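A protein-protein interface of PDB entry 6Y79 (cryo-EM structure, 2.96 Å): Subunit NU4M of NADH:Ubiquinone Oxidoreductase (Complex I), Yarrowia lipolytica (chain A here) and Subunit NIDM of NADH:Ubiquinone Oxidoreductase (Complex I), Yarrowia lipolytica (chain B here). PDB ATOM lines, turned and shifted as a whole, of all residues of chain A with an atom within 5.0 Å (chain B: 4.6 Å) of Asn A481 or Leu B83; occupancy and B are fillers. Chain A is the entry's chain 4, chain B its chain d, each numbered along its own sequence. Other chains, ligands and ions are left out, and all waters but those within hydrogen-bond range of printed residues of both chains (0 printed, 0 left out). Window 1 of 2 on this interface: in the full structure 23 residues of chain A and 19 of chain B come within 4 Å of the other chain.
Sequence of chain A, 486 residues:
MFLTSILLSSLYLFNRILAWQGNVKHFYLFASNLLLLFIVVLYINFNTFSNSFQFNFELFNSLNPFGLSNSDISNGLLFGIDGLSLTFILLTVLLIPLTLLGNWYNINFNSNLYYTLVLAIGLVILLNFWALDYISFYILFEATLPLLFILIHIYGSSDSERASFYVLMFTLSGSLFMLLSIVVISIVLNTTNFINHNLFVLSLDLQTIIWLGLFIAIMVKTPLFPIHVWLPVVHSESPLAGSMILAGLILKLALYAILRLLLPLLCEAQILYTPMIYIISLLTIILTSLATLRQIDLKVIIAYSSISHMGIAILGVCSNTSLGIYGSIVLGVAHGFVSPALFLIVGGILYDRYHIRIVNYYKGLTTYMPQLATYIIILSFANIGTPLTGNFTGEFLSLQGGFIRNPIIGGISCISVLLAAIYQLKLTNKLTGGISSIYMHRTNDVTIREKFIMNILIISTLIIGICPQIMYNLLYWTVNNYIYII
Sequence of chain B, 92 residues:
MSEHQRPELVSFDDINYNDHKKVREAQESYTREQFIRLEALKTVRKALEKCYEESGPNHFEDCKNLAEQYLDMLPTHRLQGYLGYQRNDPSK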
ATOM      1  N   ASN A  51     -19.008   8.747 -27.647  1.00  0.00           N
ATOM      2  CA  ASN A  51     -19.473   7.623 -26.847  1.00  0.00           C
ATOM      3  C   ASN A  51     -19.388   6.304 -27.603  1.00  0.00           C
ATOM      4  O   ASN A  51     -19.356   5.243 -26.974  1.00  0.00           O
ATOM      5  CB  ASN A  51     -20.913   7.888 -26.417  1.00  0.00           C
ATOM      6  CG  ASN A  51     -21.367   7.006 -25.278  1.00  0.00           C
ATOM      7  OD1 ASN A  51     -20.574   6.314 -24.643  1.00  0.00           O
ATOM      8  ND2 ASN A  51     -22.667   7.023 -25.016  1.00  0.00           N
ATOM      9  N   ASN A 198     -29.085  -1.786 -25.056  1.00  0.00           N
ATOM     10  CA  ASN A 198     -29.865  -0.977 -24.131  1.00  0.00           C
ATOM     11  C   ASN A 198     -31.188  -0.523 -24.732  1.00  0.00           C
ATOM     12  O   ASN A 198     -32.064  -0.082 -23.989  1.00  0.00           O
ATOM     13  CB  ASN A 198     -29.054   0.228 -23.652  1.00  0.00           C
ATOM     14  CG  ASN A 198     -28.455   1.039 -24.784  1.00  0.00           C
ATOM     15  OD1 ASN A 198     -28.693   0.777 -25.959  1.00  0.00           O
ATOM     16  ND2 ASN A 198     -27.667   2.037 -24.425  1.00  0.00           N
ATOM     17  N   LEU A 263     -25.749  -4.273 -16.502  1.00  0.00           N
ATOM     18  CA  LEU A 263     -26.303  -2.941 -16.310  1.00  0.00           C
ATOM     19  C   LEU A 263     -27.018  -2.320 -17.515  1.00  0.00           C
ATOM     20  O   LEU A 263     -27.902  -1.482 -17.271  1.00  0.00           O
ATOM     21  CB  LEU A 263     -25.190  -2.015 -15.803  1.00  0.00           C
ATOM     22  CG  LEU A 263     -24.719  -2.382 -14.396  1.00  0.00           C
ATOM     23  CD1 LEU A 263     -23.641  -1.448 -13.925  1.00  0.00           C
ATOM     24  CD2 LEU A 263     -25.871  -2.382 -13.420  1.00  0.00           C
ATOM     25  N   PRO A 264     -26.712  -2.622 -18.803  1.00  0.00           N
ATOM     26  CA  PRO A 264     -27.557  -2.035 -19.855  1.00  0.00           C
ATOM     27  C   PRO A 264     -28.940  -2.637 -20.064  1.00  0.00           C
ATOM     28  O   PRO A 264     -29.893  -1.861 -20.167  1.00  0.00           O
ATOM     29  CB  PRO A 264     -26.708  -2.205 -21.111  1.00  0.00           C
ATOM     30  CG  PRO A 264     -25.362  -2.238 -20.627  1.00  0.00           C
ATOM     31  CD  PRO A 264     -25.415  -3.016 -19.386  1.00  0.00           C
ATOM     32  N   CYS A 267     -31.796  -3.250 -16.292  1.00  0.00           N
ATOM     33  CA  CYS A 267     -31.924  -2.109 -15.382  1.00  0.00           C
ATOM     34  C   CYS A 267     -33.062  -2.303 -14.388  1.00  0.00           C
ATOM     35  O   CYS A 267     -32.871  -2.223 -13.162  1.00  0.00           O
ATOM     36  CB  CYS A 267     -32.180  -0.843 -16.190  1.00  0.00           C
ATOM     37  SG  CYS A 267     -30.904  -0.387 -17.349  1.00  0.00           S
ATOM     38  N   TRP A 477     -17.790   9.249 -20.221  1.00  0.00           N
ATOM     39  CA  TRP A 477     -18.987   8.722 -20.854  1.00  0.00           C
ATOM     40  C   TRP A 477     -19.528   7.551 -20.060  1.00  0.00           C
ATOM     41  O   TRP A 477     -20.688   7.555 -19.639  1.00  0.00           O
ATOM     42  CB  TRP A 477     -18.687   8.290 -22.287  1.00  0.00           C
ATOM     43  CG  TRP A 477     -18.328   9.398 -23.189  1.00  0.00           C
ATOM     44  CD1 TRP A 477     -17.103   9.664 -23.696  1.00  0.00           C
ATOM     45  CD2 TRP A 477     -19.202  10.401 -23.700  1.00  0.00           C
ATOM     46  NE1 TRP A 477     -17.153  10.771 -24.497  1.00  0.00           N
ATOM     47  CE2 TRP A 477     -18.436  11.245 -24.513  1.00  0.00           C
ATOM     48  CE3 TRP A 477     -20.561  10.670 -23.547  1.00  0.00           C
ATOM     49  CZ2 TRP A 477     -18.978  12.336 -25.173  1.00  0.00           C
ATOM     50  CZ3 TRP A 477     -21.096  11.751 -24.208  1.00  0.00           C
ATOM     51  CH2 TRP A 477     -20.308  12.571 -25.005  1.00  0.00           C
ATOM     52  N   THR A 478     -18.680   6.555 -19.807  1.00  0.00           N
ATOM     53  CA  THR A 478     -19.108   5.282 -19.248  1.00  0.00           C
ATOM     54  C   THR A 478     -19.479   5.373 -17.783  1.00  0.00           C
ATOM     55  O   THR A 478     -20.029   4.420 -17.234  1.00  0.00           O
ATOM     56  CB  THR A 478     -18.009   4.240 -19.433  1.00  0.00           C
ATOM     57  OG1 THR A 478     -16.878   4.593 -18.636  1.00  0.00           O
ATOM     58  CG2 THR A 478     -17.586   4.192 -20.887  1.00  0.00           C
ATOM     59  N   VAL A 479     -19.183   6.494 -17.147  1.00  0.00           N
ATOM     60  CA  VAL A 479     -19.608   6.738 -15.785  1.00  0.00           C
ATOM     61  C   VAL A 479     -21.047   7.247 -15.775  1.00  0.00           C
ATOM     62  O   VAL A 479     -21.808   6.972 -14.840  1.00  0.00           O
ATOM     63  CB  VAL A 479     -18.569   7.689 -15.162  1.00  0.00           C
ATOM     64  CG1 VAL A 479     -19.096   8.469 -14.033  1.00  0.00           C
ATOM     65  CG2 VAL A 479     -17.364   6.885 -14.701  1.00  0.00           C
ATOM     66  N   ASN A 480     -21.471   7.905 -16.858  1.00  0.00           N
ATOM     67  CA  ASN A 480     -22.863   8.311 -17.027  1.00  0.00           C
ATOM     68  C   ASN A 480     -23.705   7.249 -17.734  1.00  0.00           C
ATOM     69  O   ASN A 480     -24.935   7.295 -17.650  1.00  0.00           O
ATOM     70  CB  ASN A 480     -22.923   9.622 -17.808  1.00  0.00           C
ATOM     71  CG  ASN A 480     -24.235  10.350 -17.631  1.00  0.00           C
ATOM     72  OD1 ASN A 480     -25.016  10.039 -16.740  1.00  0.00           O
ATOM     73  ND2 ASN A 480     -24.493  11.310 -18.496  1.00  0.00           N
ATOM     74  N   ASN A 481     -23.069   6.292 -18.418  1.00  0.00           N
ATOM     75  CA  ASN A 481     -23.781   5.388 -19.322  1.00  0.00           C
ATOM     76  C   ASN A 481     -24.694   4.422 -18.584  1.00  0.00           C
ATOM     77  O   ASN A 481     -25.763   4.065 -19.087  1.00  0.00           O
ATOM     78  CB  ASN A 481     -22.788   4.585 -20.156  1.00  0.00           C
ATOM     79  CG  ASN A 481     -22.298   5.330 -21.361  1.00  0.00           C
ATOM     80  OD1 ASN A 481     -22.869   6.338 -21.761  1.00  0.00           O
ATOM     81  ND2 ASN A 481     -21.236   4.828 -21.962  1.00  0.00           N
ATOM     82  N   TYR A 482     -24.287   3.969 -17.404  1.00  0.00           N
ATOM     83  CA  TYR A 482     -24.925   2.842 -16.740  1.00  0.00           C
ATOM     84  C   TYR A 482     -25.836   3.266 -15.600  1.00  0.00           C
ATOM     85  O   TYR A 482     -26.238   2.425 -14.794  1.00  0.00           O
ATOM     86  CB  TYR A 482     -23.855   1.876 -16.242  1.00  0.00           C
ATOM     87  CG  TYR A 482     -23.056   1.317 -17.382  1.00  0.00           C
ATOM     88  CD1 TYR A 482     -23.593   0.352 -18.202  1.00  0.00           C
ATOM     89  CD2 TYR A 482     -21.784   1.784 -17.667  1.00  0.00           C
ATOM     90  CE1 TYR A 482     -22.886  -0.149 -19.256  1.00  0.00           C
ATOM     91  CE2 TYR A 482     -21.069   1.285 -18.731  1.00  0.00           C
ATOM     92  CZ  TYR A 482     -21.629   0.316 -19.519  1.00  0.00           C
ATOM     93  OH  TYR A 482     -20.934  -0.205 -20.581  1.00  0.00           O
ATOM     94  N   ILE A 483     -26.181   4.537 -15.526  1.00  0.00           N
ATOM     95  CA  ILE A 483     -26.967   5.075 -14.425  1.00  0.00           C
ATOM     96  C   ILE A 483     -28.429   5.093 -14.845  1.00  0.00           C
ATOM     97  O   ILE A 483     -28.758   5.484 -15.970  1.00  0.00           O
ATOM     98  CB  ILE A 483     -26.460   6.477 -14.038  1.00  0.00           C
ATOM     99  CG1 ILE A 483     -24.957   6.449 -13.769  1.00  0.00           C
ATOM    100  CG2 ILE A 483     -27.150   6.987 -12.808  1.00  0.00           C
ATOM    101  CD1 ILE A 483     -24.528   5.445 -12.727  1.00  0.00           C
ATOM    102  N   TYR A 484     -29.311   4.659 -13.942  1.00  0.00           N
ATOM    103  CA  TYR A 484     -30.745   4.528 -14.204  1.00  0.00           C
ATOM    104  C   TYR A 484     -31.493   5.265 -13.088  1.00  0.00           C
ATOM    105  O   TYR A 484     -31.979   4.654 -12.137  1.00  0.00           O
ATOM    106  CB  TYR A 484     -31.096   3.037 -14.272  1.00  0.00           C
ATOM    107  CG  TYR A 484     -32.507   2.711 -14.667  1.00  0.00           C
ATOM    108  CD1 TYR A 484     -32.897   2.727 -15.995  1.00  0.00           C
ATOM    109  CD2 TYR A 484     -33.449   2.365 -13.710  1.00  0.00           C
ATOM    110  CE1 TYR A 484     -34.182   2.426 -16.354  1.00  0.00           C
ATOM    111  CE2 TYR A 484     -34.739   2.067 -14.061  1.00  0.00           C
ATOM    112  CZ  TYR A 484     -35.098   2.099 -15.385  1.00  0.00           C
ATOM    113  OH  TYR A 484     -36.385   1.802 -15.750  1.00  0.00           O
ATOM    114  N   GLY B  81     -28.070   9.942 -16.021  1.00  0.00           N
ATOM    115  CA  GLY B  81     -28.096   8.824 -16.939  1.00  0.00           C
ATOM    116  C   GLY B  81     -29.191   8.923 -17.976  1.00  0.00           C
ATOM    117  O   GLY B  81     -30.326   9.289 -17.657  1.00  0.00           O
ATOM    118  N   TYR B  82     -28.865   8.595 -19.225  1.00  0.00           N
ATOM    119  CA  TYR B  82     -29.852   8.627 -20.294  1.00  0.00           C
ATOM    120  C   TYR B  82     -30.790   7.437 -20.264  1.00  0.00           C
ATOM    121  O   TYR B  82     -31.863   7.509 -20.874  1.00  0.00           O
ATOM    122  CB  TYR B  82     -29.155   8.696 -21.655  1.00  0.00           C
ATOM    123  CG  TYR B  82     -28.230   7.539 -21.961  1.00  0.00           C
ATOM    124  CD1 TYR B  82     -28.705   6.373 -22.552  1.00  0.00           C
ATOM    125  CD2 TYR B  82     -26.876   7.624 -21.686  1.00  0.00           C
ATOM    126  CE1 TYR B  82     -27.877   5.329 -22.821  1.00  0.00           C
ATOM    127  CE2 TYR B  82     -26.037   6.579 -21.970  1.00  0.00           C
ATOM    128  CZ  TYR B  82     -26.547   5.434 -22.531  1.00  0.00           C
ATOM    129  OH  TYR B  82     -25.722   4.379 -22.828  1.00  0.00           O
ATOM    130  N   LEU B  83     -30.376   6.343 -19.614  1.00  0.00           N
ATOM    131  CA  LEU B  83     -31.127   5.092 -19.643  1.00  0.00           C
ATOM    132  C   LEU B  83     -32.495   5.252 -19.024  1.00  0.00           C
ATOM    133  O   LEU B  83     -33.478   4.737 -19.550  1.00  0.00           O
ATOM    134  CB  LEU B  83     -30.369   3.990 -18.908  1.00  0.00           C
ATOM    135  CG  LEU B  83     -29.154   3.330 -19.542  1.00  0.00           C
ATOM    136  CD1 LEU B  83     -28.603   2.317 -18.580  1.00  0.00           C
ATOM    137  CD2 LEU B  83     -29.531   2.667 -20.843  1.00  0.00           C
ATOM    138  N   GLY B  84     -32.587   5.988 -17.924  1.00  0.00           N
ATOM    139  CA  GLY B  84     -33.858   6.102 -17.240  1.00  0.00           C
ATOM    140  C   GLY B  84     -34.908   6.865 -18.019  1.00  0.00           C
ATOM    141  O   GLY B  84     -36.101   6.597 -17.875  1.00  0.00           O
ATOM    142  N   TYR B  85     -34.489   7.798 -18.870  1.00  0.00           N
ATOM    143  CA  TYR B  85     -35.450   8.481 -19.720  1.00  0.00           C
ATOM    144  C   TYR B  85     -35.673   7.770 -21.045  1.00  0.00           C
ATOM    145  O   TYR B  85     -36.760   7.880 -21.616  1.00  0.00           O
ATOM    146  CB  TYR B  85     -35.016   9.924 -19.993  1.00  0.00           C
ATOM    147  CG  TYR B  85     -36.083  10.729 -20.700  1.00  0.00           C
ATOM    148  CD1 TYR B  85     -37.238  11.118 -20.035  1.00  0.00           C
ATOM    149  CD2 TYR B  85     -35.951  11.069 -22.037  1.00  0.00           C
ATOM    150  CE1 TYR B  85     -38.220  11.835 -20.677  1.00  0.00           C
ATOM    151  CE2 TYR B  85     -36.929  11.785 -22.687  1.00  0.00           C
ATOM    152  CZ  TYR B  85     -38.061  12.163 -22.000  1.00  0.00           C
ATOM    153  OH  TYR B  85     -39.037  12.876 -22.646  1.00  0.00           O
ATOM    154  N   GLN B  86     -34.687   7.045 -21.564  1.00  0.00           N
ATOM    155  CA  GLN B  86     -34.899   6.407 -22.852  1.00  0.00           C
ATOM    156  C   GLN B  86     -35.571   5.044 -22.753  1.00  0.00           C
ATOM    157  O   GLN B  86     -36.115   4.571 -23.751  1.00  0.00           O
ATOM    158  CB  GLN B  86     -33.582   6.276 -23.611  1.00  0.00           C
ATOM    159  CG  GLN B  86     -32.805   5.037 -23.303  1.00  0.00           C
ATOM    160  CD  GLN B  86     -31.705   4.800 -24.289  1.00  0.00           C
ATOM    161  OE1 GLN B  86     -31.497   5.591 -25.196  1.00  0.00           O
ATOM    162  NE2 GLN B  86     -30.982   3.711 -24.117  1.00  0.00           N
ATOM    163  N   ARG B  87     -35.562   4.401 -21.587  1.00  0.00           N
ATOM    164  CA  ARG B  87     -36.265   3.136 -21.448  1.00  0.00           C
ATOM    165  C   ARG B  87     -37.721   3.329 -21.081  1.00  0.00           C
ATOM    166  O   ARG B  87     -38.518   2.411 -21.274  1.00  0.00           O
ATOM    167  CB  ARG B  87     -35.615   2.251 -20.378  1.00  0.00           C
ATOM    168  CG  ARG B  87     -34.165   1.865 -20.602  1.00  0.00           C
ATOM    169  CD  ARG B  87     -34.006   0.734 -21.527  1.00  0.00           C
ATOM    170  NE  ARG B  87     -34.631  -0.456 -20.987  1.00  0.00           N
ATOM    171  CZ  ARG B  87     -33.980  -1.451 -20.409  1.00  0.00           C
ATOM    172  NH1 ARG B  87     -32.671  -1.402 -20.301  1.00  0.00           N
ATOM    173  NH2 ARG B  87     -34.644  -2.497 -19.949  1.00  0.00           N
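Among the printed residues, pairs that only touch across the chains: Asn A198 with Leu B83 (3.8 Å), Asn A198 with Gln B86 (3.7 Å), Asn A198 with Arg B87 (3.2 Å), Cys A267 with Leu B83 (3.8 Å), Asn A481 with Tyr B82 (3.2 Å), Asn A481 with Leu B83 (3.4 Å), Ile A483 with Gly B81 (3.5 Å), Ile A483 with Leu B83 (3.7 Å), Tyr A484 with Leu B83 (3.96 Å) and Tyr A484 with Gly B84 (3.7 Å).
ND2 of Asn A481 is in hydrogen-bond range of OD1 of Asn A51 (3.1 Å). O of Leu A263 sits at hydrogen-bond distance from SG of Cys A267 (3.2 Å). O of Pro A264 sits at hydrogen-bond distance from SG of Cys A267 (3.3 Å). OD1 of Asn A481 sits close to O of Trp A477, at 3.3 Å.
Of the 7 printed residues of chain B, 6 touch a printed residue of chain A. Hydrophobic or aromatic side chains of chain B that line the printed part of chain A: Tyr B82 and Leu B83. Among the printed residues, 14 pairs touch across the chains.
The side-chain amide oxygen (OD1) of Asn A480 lies within hydrogen-bond range of the backbone NH (N) of Gly B81 (3.1 Å). ND2 of Asn A198 sits at hydrogen-bond distance from OH of Tyr B82, at 3.4 Å. The backbone carbonyl oxygen (O) of Pro A264 is in hydrogen-bond range of the guanidinium group (NH1) of Arg B87 (2.8 Å). NH1 of Arg B87 sits at hydrogen-bond distance from SG of Cys A267.
Asn A51 touches none of the printed residues of chain B. Of the printed residues of chain B, Cys A267 touches Leu B83 (3.8 Å) and Arg B87 (3.6 Å). Of chain B, only Tyr B82 and Leu B83 come within 4 Å of Asn A481. Of the printed residues of chain A, Gly B81 touches Asn A480 (3.1 Å) and Ile A483 (3.5 Å). Of the printed residues of chain A, Arg B87 touches Asn A198, Pro A264 and Cys A267. The nearest printed residue of chain A that does not touch Gly B81 is Tyr A484 (5.3 Å).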
